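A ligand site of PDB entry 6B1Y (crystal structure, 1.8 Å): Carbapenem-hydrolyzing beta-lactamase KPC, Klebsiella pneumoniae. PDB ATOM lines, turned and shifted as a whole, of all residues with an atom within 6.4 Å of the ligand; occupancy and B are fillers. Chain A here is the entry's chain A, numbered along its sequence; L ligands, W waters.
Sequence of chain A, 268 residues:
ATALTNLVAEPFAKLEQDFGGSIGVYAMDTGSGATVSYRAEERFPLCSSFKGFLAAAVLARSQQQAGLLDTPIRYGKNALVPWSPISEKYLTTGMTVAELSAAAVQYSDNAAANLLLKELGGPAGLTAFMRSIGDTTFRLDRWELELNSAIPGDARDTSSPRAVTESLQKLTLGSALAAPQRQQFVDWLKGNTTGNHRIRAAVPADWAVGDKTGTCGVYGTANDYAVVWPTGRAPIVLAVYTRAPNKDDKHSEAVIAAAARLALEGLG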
ATOM      1  N   LEU A  46       1.324 -12.779  19.714  1.00  0.00           N
ATOM      2  CA  LEU A  46      -0.050 -12.575  20.056  1.00  0.00           C
ATOM      3  C   LEU A  46      -0.361 -11.142  20.412  1.00  0.00           C
ATOM      4  O   LEU A  46      -1.462 -10.649  20.062  1.00  0.00           O
ATOM      5  CB  LEU A  46      -0.429 -13.481  21.235  1.00  0.00           C
ATOM      6  CG  LEU A  46      -0.482 -14.943  20.778  1.00  0.00           C
ATOM      7  CD1 LEU A  46      -0.334 -15.868  21.972  1.00  0.00           C
ATOM      8  CD2 LEU A  46      -1.768 -15.205  20.014  1.00  0.00           C
ATOM      9  N   CYS A  47       0.562 -10.484  21.118  1.00  0.00           N
ATOM     10  CA  CYS A  47       0.243  -9.181  21.723  1.00  0.00           C
ATOM     11  C   CYS A  47      -1.070  -9.270  22.557  1.00  0.00           C
ATOM     12  O   CYS A  47      -1.296 -10.281  23.187  1.00  0.00           O
ATOM     13  CB  CYS A  47       0.202  -8.068  20.632  1.00  0.00           C
ATOM     14  SG  CYS A  47       1.495  -8.138  19.372  1.00  0.00           S
ATOM     15  N   SER A  48      -1.971  -8.276  22.506  1.00  0.00           N
ATOM     16  CA  SER A  48      -3.220  -8.363  23.229  1.00  0.00           C
ATOM     17  C   SER A  48      -4.234  -9.388  22.754  1.00  0.00           C
ATOM     18  O   SER A  48      -5.202  -9.657  23.469  1.00  0.00           O
ATOM     19  CB  SER A  48      -3.986  -7.051  23.171  1.00  0.00           C
ATOM     20  OG  SER A  48      -3.377  -6.030  23.947  1.00  0.00           O
ATOM     21  N   SER A  49      -4.045  -9.951  21.567  1.00  0.00           N
ATOM     22  CA  SER A  49      -5.036 -10.847  20.994  1.00  0.00           C
ATOM     23  C   SER A  49      -5.203 -12.153  21.825  1.00  0.00           C
ATOM     24  O   SER A  49      -6.196 -12.838  21.693  1.00  0.00           O
ATOM     25  CB  SER A  49      -4.702 -11.164  19.559  1.00  0.00           C
ATOM     26  OG  SER A  49      -3.632 -12.100  19.479  1.00  0.00           O
ATOM     27  N   LYS A  51      -6.171 -12.202  24.737  1.00  0.00           N
ATOM     28  CA  LYS A  51      -7.245 -11.881  25.658  1.00  0.00           C
ATOM     29  C   LYS A  51      -8.590 -12.483  25.268  1.00  0.00           C
ATOM     30  O   LYS A  51      -9.397 -12.765  26.155  1.00  0.00           O
ATOM     31  CB  LYS A  51      -7.350 -10.366  25.844  1.00  0.00           C
ATOM     32  CG  LYS A  51      -6.131  -9.811  26.565  1.00  0.00           C
ATOM     33  CD  LYS A  51      -6.054  -8.298  26.428  1.00  0.00           C
ATOM     34  CE  LYS A  51      -4.817  -7.864  27.157  1.00  0.00           C
ATOM     35  NZ  LYS A  51      -4.363  -6.498  26.823  1.00  0.00           N
ATOM     36  N   PRO A  82       0.044   0.154  32.660  1.00  0.00           N
ATOM     37  CA  PRO A  82      -0.531   1.033  31.682  1.00  0.00           C
ATOM     38  C   PRO A  82      -1.374   0.244  30.635  1.00  0.00           C
ATOM     39  O   PRO A  82      -1.215  -0.967  30.476  1.00  0.00           O
ATOM     40  CB  PRO A  82       0.669   1.717  31.036  1.00  0.00           C
ATOM     41  CG  PRO A  82       1.888   1.178  31.663  1.00  0.00           C
ATOM     42  CD  PRO A  82       1.492   0.365  32.857  1.00  0.00           C
ATOM     43  N   TRP A  83      -2.271   0.979  29.970  1.00  0.00           N
ATOM     44  CA  TRP A  83      -3.349   0.443  29.093  1.00  0.00           C
ATOM     45  C   TRP A  83      -4.279  -0.516  29.849  1.00  0.00           C
ATOM     46  O   TRP A  83      -4.576  -1.638  29.406  1.00  0.00           O
ATOM     47  CB  TRP A  83      -2.817  -0.206  27.831  1.00  0.00           C
ATOM     48  CG  TRP A  83      -2.040   0.686  26.906  1.00  0.00           C
ATOM     49  CD1 TRP A  83      -2.545   1.425  25.911  1.00  0.00           C
ATOM     50  CD2 TRP A  83      -0.611   0.871  26.866  1.00  0.00           C
ATOM     51  NE1 TRP A  83      -1.544   2.082  25.238  1.00  0.00           N
ATOM     52  CE2 TRP A  83      -0.348   1.781  25.832  1.00  0.00           C
ATOM     53  CE3 TRP A  83       0.464   0.414  27.640  1.00  0.00           C
ATOM     54  CZ2 TRP A  83       0.955   2.196  25.503  1.00  0.00           C
ATOM     55  CZ3 TRP A  83       1.761   0.826  27.279  1.00  0.00           C
ATOM     56  CH2 TRP A  83       1.975   1.704  26.240  1.00  0.00           C
ATOM     57  N   SER A  84      -4.796  -0.010  30.934  1.00  0.00           N
ATOM     58  CA  SER A  84      -5.761  -0.706  31.737  1.00  0.00           C
ATOM     59  C   SER A  84      -6.869   0.299  32.145  1.00  0.00           C
ATOM     60  O   SER A  84      -7.039   0.573  33.349  1.00  0.00           O
ATOM     61  CB  SER A  84      -5.058  -1.234  32.978  1.00  0.00           C
ATOM     62  OG  SER A  84      -4.069  -2.199  32.705  1.00  0.00           O
ATOM     63  N   PRO A  85      -7.607   0.863  31.163  1.00  0.00           N
ATOM     64  CA  PRO A  85      -8.495   2.014  31.385  1.00  0.00           C
ATOM     65  C   PRO A  85      -9.705   1.637  32.262  1.00  0.00           C
ATOM     66  O   PRO A  85     -10.158   2.478  33.058  1.00  0.00           O
ATOM     67  CB  PRO A  85      -8.938   2.387  29.975  1.00  0.00           C
ATOM     68  CG  PRO A  85      -8.815   1.116  29.184  1.00  0.00           C
ATOM     69  CD  PRO A  85      -7.541   0.531  29.742  1.00  0.00           C
ATOM     70  N   TYR A 107     -11.928  -3.655  25.610  1.00  0.00           N
ATOM     71  CA  TYR A 107     -11.032  -2.511  25.777  1.00  0.00           C
ATOM     72  C   TYR A 107      -9.583  -2.942  25.833  1.00  0.00           C
ATOM     73  O   TYR A 107      -8.698  -2.114  25.997  1.00  0.00           O
ATOM     74  CB  TYR A 107     -11.414  -1.758  27.076  1.00  0.00           C
ATOM     75  CG  TYR A 107     -12.715  -1.061  26.834  1.00  0.00           C
ATOM     76  CD1 TYR A 107     -12.744   0.188  26.199  1.00  0.00           C
ATOM     77  CD2 TYR A 107     -13.921  -1.673  27.150  1.00  0.00           C
ATOM     78  CE1 TYR A 107     -13.959   0.833  25.908  1.00  0.00           C
ATOM     79  CE2 TYR A 107     -15.130  -1.055  26.870  1.00  0.00           C
ATOM     80  CZ  TYR A 107     -15.157   0.187  26.265  1.00  0.00           C
ATOM     81  OH  TYR A 107     -16.378   0.775  25.935  1.00  0.00           O
ATOM     82  N   SER A 108      -9.322  -4.230  25.724  1.00  0.00           N
ATOM     83  CA  SER A 108      -7.961  -4.720  25.713  1.00  0.00           C
ATOM     84  C   SER A 108      -7.232  -4.367  27.000  1.00  0.00           C
ATOM     85  O   SER A 108      -6.009  -4.123  27.021  1.00  0.00           O
ATOM     86  CB  SER A 108      -7.230  -4.219  24.481  1.00  0.00           C
ATOM     87  OG  SER A 108      -6.271  -5.151  24.097  1.00  0.00           O
ATOM     88  N   ASP A 109      -7.966  -4.388  28.106  1.00  0.00           N
ATOM     89  CA  ASP A 109      -7.445  -3.912  29.353  1.00  0.00           C
ATOM     90  C   ASP A 109      -6.348  -4.869  29.825  1.00  0.00           C
ATOM     91  O   ASP A 109      -6.596  -6.066  29.998  1.00  0.00           O
ATOM     92  CB  ASP A 109      -8.591  -3.862  30.353  1.00  0.00           C
ATOM     93  CG  ASP A 109      -8.246  -3.230  31.672  1.00  0.00           C
ATOM     94  OD1 ASP A 109      -8.915  -2.217  31.991  1.00  0.00           O
ATOM     95  OD2 ASP A 109      -7.396  -3.738  32.432  1.00  0.00           O
ATOM     96  N   ASN A 110      -5.155  -4.329  30.070  1.00  0.00           N
ATOM     97  CA  ASN A 110      -3.985  -5.164  30.480  1.00  0.00           C
ATOM     98  C   ASN A 110      -4.074  -5.796  31.882  1.00  0.00           C
ATOM     99  O   ASN A 110      -3.918  -7.016  32.035  1.00  0.00           O
ATOM    100  CB  ASN A 110      -2.672  -4.378  30.352  1.00  0.00           C
ATOM    101  CG  ASN A 110      -2.162  -4.321  28.926  1.00  0.00           C
ATOM    102  OD1 ASN A 110      -2.496  -5.173  28.131  1.00  0.00           O
ATOM    103  ND2 ASN A 110      -1.363  -3.308  28.581  1.00  0.00           N
ATOM    104  N   GLU A 144       1.266  -9.438  30.991  1.00  0.00           N
ATOM    105  CA  GLU A 144       1.344  -8.037  30.603  1.00  0.00           C
ATOM    106  C   GLU A 144       2.338  -7.304  31.522  1.00  0.00           C
ATOM    107  O   GLU A 144       2.278  -7.475  32.757  1.00  0.00           O
ATOM    108  CB  GLU A 144      -0.040  -7.371  30.626  1.00  0.00           C
ATOM    109  CG  GLU A 144      -1.001  -7.953  29.591  1.00  0.00           C
ATOM    110  CD  GLU A 144      -0.656  -7.514  28.187  1.00  0.00           C
ATOM    111  OE1 GLU A 144       0.362  -6.782  28.047  1.00  0.00           O
ATOM    112  OE2 GLU A 144      -1.416  -7.846  27.232  1.00  0.00           O
ATOM    113  N   LEU A 145       3.263  -6.513  30.977  1.00  0.00           N
ATOM    114  CA  LEU A 145       3.414  -6.099  29.579  1.00  0.00           C
ATOM    115  C   LEU A 145       4.537  -6.806  28.832  1.00  0.00           C
ATOM    116  O   LEU A 145       4.735  -6.568  27.614  1.00  0.00           O
ATOM    117  CB  LEU A 145       3.776  -4.611  29.543  1.00  0.00           C
ATOM    118  CG  LEU A 145       2.802  -3.604  30.104  1.00  0.00           C
ATOM    119  CD1 LEU A 145       3.505  -2.280  30.436  1.00  0.00           C
ATOM    120  CD2 LEU A 145       1.782  -3.293  29.071  1.00  0.00           C
ATOM    121  N   GLU A 146       5.276  -7.693  29.503  1.00  0.00           N
ATOM    122  CA  GLU A 146       6.480  -8.275  28.903  1.00  0.00           C
ATOM    123  C   GLU A 146       6.199  -9.140  27.671  1.00  0.00           C
ATOM    124  O   GLU A 146       7.074  -9.268  26.798  1.00  0.00           O
ATOM    125  CB  GLU A 146       7.248  -9.104  29.928  1.00  0.00           C
ATOM    126  CG  GLU A 146       7.779  -8.260  31.086  1.00  0.00           C
ATOM    127  CD  GLU A 146       6.839  -8.080  32.268  1.00  0.00           C
ATOM    128  OE1 GLU A 146       5.649  -8.521  32.268  1.00  0.00           O
ATOM    129  OE2 GLU A 146       7.327  -7.450  33.233  1.00  0.00           O
ATOM    130  N   ASN A 148       4.533  -8.525  25.199  1.00  0.00           N
ATOM    131  CA  ASN A 148       4.519  -7.708  23.954  1.00  0.00           C
ATOM    132  C   ASN A 148       5.871  -7.456  23.295  1.00  0.00           C
ATOM    133  O   ASN A 148       5.900  -6.730  22.327  1.00  0.00           O
ATOM    134  CB  ASN A 148       3.908  -6.322  24.279  1.00  0.00           C
ATOM    135  CG  ASN A 148       2.491  -6.440  24.727  1.00  0.00           C
ATOM    136  OD1 ASN A 148       1.645  -6.840  23.936  1.00  0.00           O
ATOM    137  ND2 ASN A 148       2.214  -6.117  25.987  1.00  0.00           N
ATOM    138  N   SER A 149       6.978  -8.033  23.793  1.00  0.00           N
ATOM    139  CA  SER A 149       8.299  -7.600  23.319  1.00  0.00           C
ATOM    140  C   SER A 149       8.519  -7.880  21.838  1.00  0.00           C
ATOM    141  O   SER A 149       9.233  -7.150  21.170  1.00  0.00           O
ATOM    142  CB  SER A 149       9.429  -8.208  24.177  1.00  0.00           C
ATOM    143  OG  SER A 149       9.313  -9.603  24.190  1.00  0.00           O
ATOM    144  N   THR A 194     -12.144  -1.849  19.951  1.00  0.00           N
ATOM    145  CA  THR A 194     -10.806  -1.497  19.454  1.00  0.00           C
ATOM    146  C   THR A 194     -10.482  -1.890  18.031  1.00  0.00           C
ATOM    147  O   THR A 194      -9.363  -1.609  17.544  1.00  0.00           O
ATOM    148  CB  THR A 194      -9.714  -2.114  20.335  1.00  0.00           C
ATOM    149  OG1 THR A 194      -9.752  -3.540  20.197  1.00  0.00           O
ATOM    150  CG2 THR A 194      -9.918  -1.692  21.791  1.00  0.00           C
ATOM    151  N   LYS A 212     -11.005  -9.621  18.139  1.00  0.00           N
ATOM    152  CA  LYS A 212     -10.030  -9.193  19.128  1.00  0.00           C
ATOM    153  C   LYS A 212      -8.722  -8.793  18.435  1.00  0.00           C
ATOM    154  O   LYS A 212      -8.167  -9.560  17.650  1.00  0.00           O
ATOM    155  CB  LYS A 212      -9.770 -10.270  20.208  1.00  0.00           C
ATOM    156  CG  LYS A 212      -8.713  -9.846  21.199  1.00  0.00           C
ATOM    157  CD  LYS A 212      -9.285  -8.904  22.229  1.00  0.00           C
ATOM    158  CE  LYS A 212      -8.232  -8.139  23.003  1.00  0.00           C
ATOM    159  NZ  LYS A 212      -7.744  -6.905  22.333  1.00  0.00           N
ATOM    160  N   THR A 213      -8.237  -7.632  18.802  1.00  0.00           N
ATOM    161  CA  THR A 213      -7.022  -7.026  18.246  1.00  0.00           C
ATOM    162  C   THR A 213      -5.805  -7.216  19.160  1.00  0.00           C
ATOM    163  O   THR A 213      -5.950  -7.546  20.317  1.00  0.00           O
ATOM    164  CB  THR A 213      -7.251  -5.512  18.131  1.00  0.00           C
ATOM    165  OG1 THR A 213      -7.568  -4.975  19.411  1.00  0.00           O
ATOM    166  CG2 THR A 213      -8.360  -5.218  17.168  1.00  0.00           C
ATOM    167  N   GLY A 214      -4.623  -6.983  18.601  1.00  0.00           N
ATOM    168  CA  GLY A 214      -3.360  -6.935  19.312  1.00  0.00           C
ATOM    169  C   GLY A 214      -2.470  -5.918  18.645  1.00  0.00           C
ATOM    170  O   GLY A 214      -2.442  -5.804  17.435  1.00  0.00           O
ATOM    171  N   THR A 215      -1.760  -5.149  19.456  1.00  0.00           N
ATOM    172  CA  THR A 215      -0.802  -4.177  18.939  1.00  0.00           C
ATOM    173  C   THR A 215       0.392  -4.180  19.858  1.00  0.00           C
ATOM    174  O   THR A 215       0.335  -3.591  20.939  1.00  0.00           O
ATOM    175  CB  THR A 215      -1.442  -2.770  18.901  1.00  0.00           C
ATOM    176  OG1 THR A 215      -2.702  -2.818  18.246  1.00  0.00           O
ATOM    177  CG2 THR A 215      -0.600  -1.816  18.086  1.00  0.00           C
ATOM    178  N   CYS A 216       1.494  -4.809  19.469  1.00  0.00           N
ATOM    179  CA  CYS A 216       2.649  -4.907  20.403  1.00  0.00           C
ATOM    180  C   CYS A 216       3.410  -3.584  20.591  1.00  0.00           C
ATOM    181  O   CYS A 216       4.151  -3.430  21.593  1.00  0.00           O
ATOM    182  CB  CYS A 216       3.631  -5.975  19.975  1.00  0.00           C
ATOM    183  SG  CYS A 216       3.181  -7.667  20.442  1.00  0.00           S
ATOM    184  N   GLY A 217       3.260  -2.669  19.640  1.00  0.00           N
ATOM    185  CA  GLY A 217       3.870  -1.319  19.691  1.00  0.00           C
ATOM    186  C   GLY A 217       5.321  -1.301  19.218  1.00  0.00           C
ATOM    187  O   GLY A 217       5.977  -0.269  19.311  1.00  0.00           O
ATOM    188  N   VAL A 218       5.815  -2.441  18.684  1.00  0.00           N
ATOM    189  CA  VAL A 218       7.176  -2.599  18.184  1.00  0.00           C
ATOM    190  C   VAL A 218       7.246  -3.604  17.035  1.00  0.00           C
ATOM    191  O   VAL A 218       6.346  -4.422  16.857  1.00  0.00           O
ATOM    192  CB  VAL A 218       8.121  -3.166  19.280  1.00  0.00           C
ATOM    193  CG1 VAL A 218       8.519  -2.046  20.222  1.00  0.00           C
ATOM    194  CG2 VAL A 218       7.520  -4.397  19.981  1.00  0.00           C
HETATM  195  O1  LIG L   1      -1.986  -5.475  22.418  1.00  0.00           O
HETATM  196  C1  LIG L   1      -2.583  -5.084  23.425  1.00  0.00           C
HETATM  197  N1  LIG L   1      -2.341  -3.899  24.021  1.00  0.00           N
HETATM  198  C2  LIG L   1      -3.216  -3.433  25.121  1.00  0.00           C
HETATM  199  C3  LIG L   1      -3.600  -2.111  24.661  1.00  0.00           C
HETATM  200  N2  LIG L   1      -4.773  -1.596  24.992  1.00  0.00           N
HETATM  201  C4  LIG L   1      -2.840  -1.261  23.828  1.00  0.00           C
HETATM  202  C5  LIG L   1      -1.920  -1.960  22.923  1.00  0.00           C
HETATM  203  C6  LIG L   1      -1.185  -3.123  23.601  1.00  0.00           C
HETATM  204  C7  LIG L   1      -0.253  -2.785  24.641  1.00  0.00           C
HETATM  205  O2  LIG L   1      -0.195  -3.434  25.706  1.00  0.00           O
HETATM  206  N3  LIG L   1       0.602  -1.743  24.365  1.00  0.00           N
HETATM  207  N4  LIG L   1       1.660  -1.569  25.136  1.00  0.00           N
HETATM  208  C8  LIG L   1       2.758  -2.337  24.914  1.00  0.00           C
HETATM  209  O3  LIG L   1       2.718  -3.313  24.193  1.00  0.00           O
HETATM  210  C9  LIG L   1       4.046  -1.879  25.633  1.00  0.00           C
HETATM  211  C10 LIG L   1       4.596  -0.644  25.041  1.00  0.00           C
HETATM  212  C11 LIG L   1       5.213  -1.260  23.692  1.00  0.00           C
HETATM  213  N5  LIG L   1       5.572  -2.691  24.012  1.00  0.00           N
HETATM  214  C12 LIG L   1       5.208  -2.858  25.437  1.00  0.00           C
HETATM  215  O   HOH W   1       1.224  -1.030  21.905  1.00  0.00           O
HETATM  216  O   HOH W   2      -6.517  -0.127  23.041  1.00  0.00           O
HETATM  217  O   HOH W   3      -0.808  -6.460  25.151  1.00  0.00           O
HETATM  218  O   HOH W   4      -6.563  -0.672  27.092  1.00  0.00           O
HETATM  219  O   HOH W   5       7.134  -5.225  25.666  1.00  0.00           O
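C1 of the ligand is bonded to OG of Ser 48 (1.3 Å). The backbone NH (N) of Ser 48 sits close to an oxygen (O1) of the ligand. N of Thr 215 is in hydrogen-bond range of O1 of the ligand. The backbone carbonyl oxygen of Ser 108 lies close to a nitrogen (N2) of the ligand, 3.5 Å away. An oxygen (O3) of the ligand lies close to the side-chain amide nitrogen (ND2) of Asn 148 (3.4 Å). An oxygen (O2) of the ligand lies within hydrogen-bond range of the side-chain amide nitrogen (ND2) of Asn 110, at 3.1 Å.
The side-chain amino group (NZ) of Lys 212 lies within hydrogen-bond range of the side-chain hydroxyl (OG) of Ser 108 (2.9 Å). The side-chain carboxylate (OE1) of Glu 144 sits at hydrogen-bond distance from the side-chain amide nitrogen (ND2) of Asn 148 (2.8 Å). The side-chain amino group (NZ) of Lys 51 sits at hydrogen-bond distance from the side-chain hydroxyl (OG) of Ser 48, 3.1 Å away. The side-chain amino group of Lys 51 lies within hydrogen-bond range of the backbone carbonyl oxygen of Ser 108, at 2.9 Å. The side-chain sulfur (SG) of Cys 216 forms a disulfide with the side-chain sulfur (SG) of Cys 47 (2.1 Å). The backbone carbonyl oxygen of Pro 82 sits at hydrogen-bond distance from the side-chain amide nitrogen of Asn 110 (3.0 Å). The side-chain carboxylate (OE2) of Glu 144 sits close to the side-chain amide oxygen (OD1) of Asn 110, at 3.0 Å. NZ of Lys 51 is in salt-bridge range of OE2 of Glu 144 (3.3 Å).
The backbone carbonyl oxygen of Cys 216 lies close to a nitrogen (N5) of the ligand (2.9 Å). Merely in contact with the ligand: Cys 47, Lys 51, Trp 83, Leu 145 and Gly 214. Within 4 Å of the ligand: Cys 47, Ser 48, Lys 51, Trp 83, Ser 108, Asn 110, Leu 145, Asn 148, Gly 214, Thr 215 and Cys 216.
Water W1 lies within hydrogen-bond range of N3 of the ligand, O of Thr 215 and N of Gly 217. Water W5 lies within hydrogen-bond range of the backbone carbonyl oxygen (O) of Leu 145 (3.4 Å), the backbone NH (N) of Ser 149 (3.4 Å) and a nitrogen (N5) of the ligand (3.4 Å).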
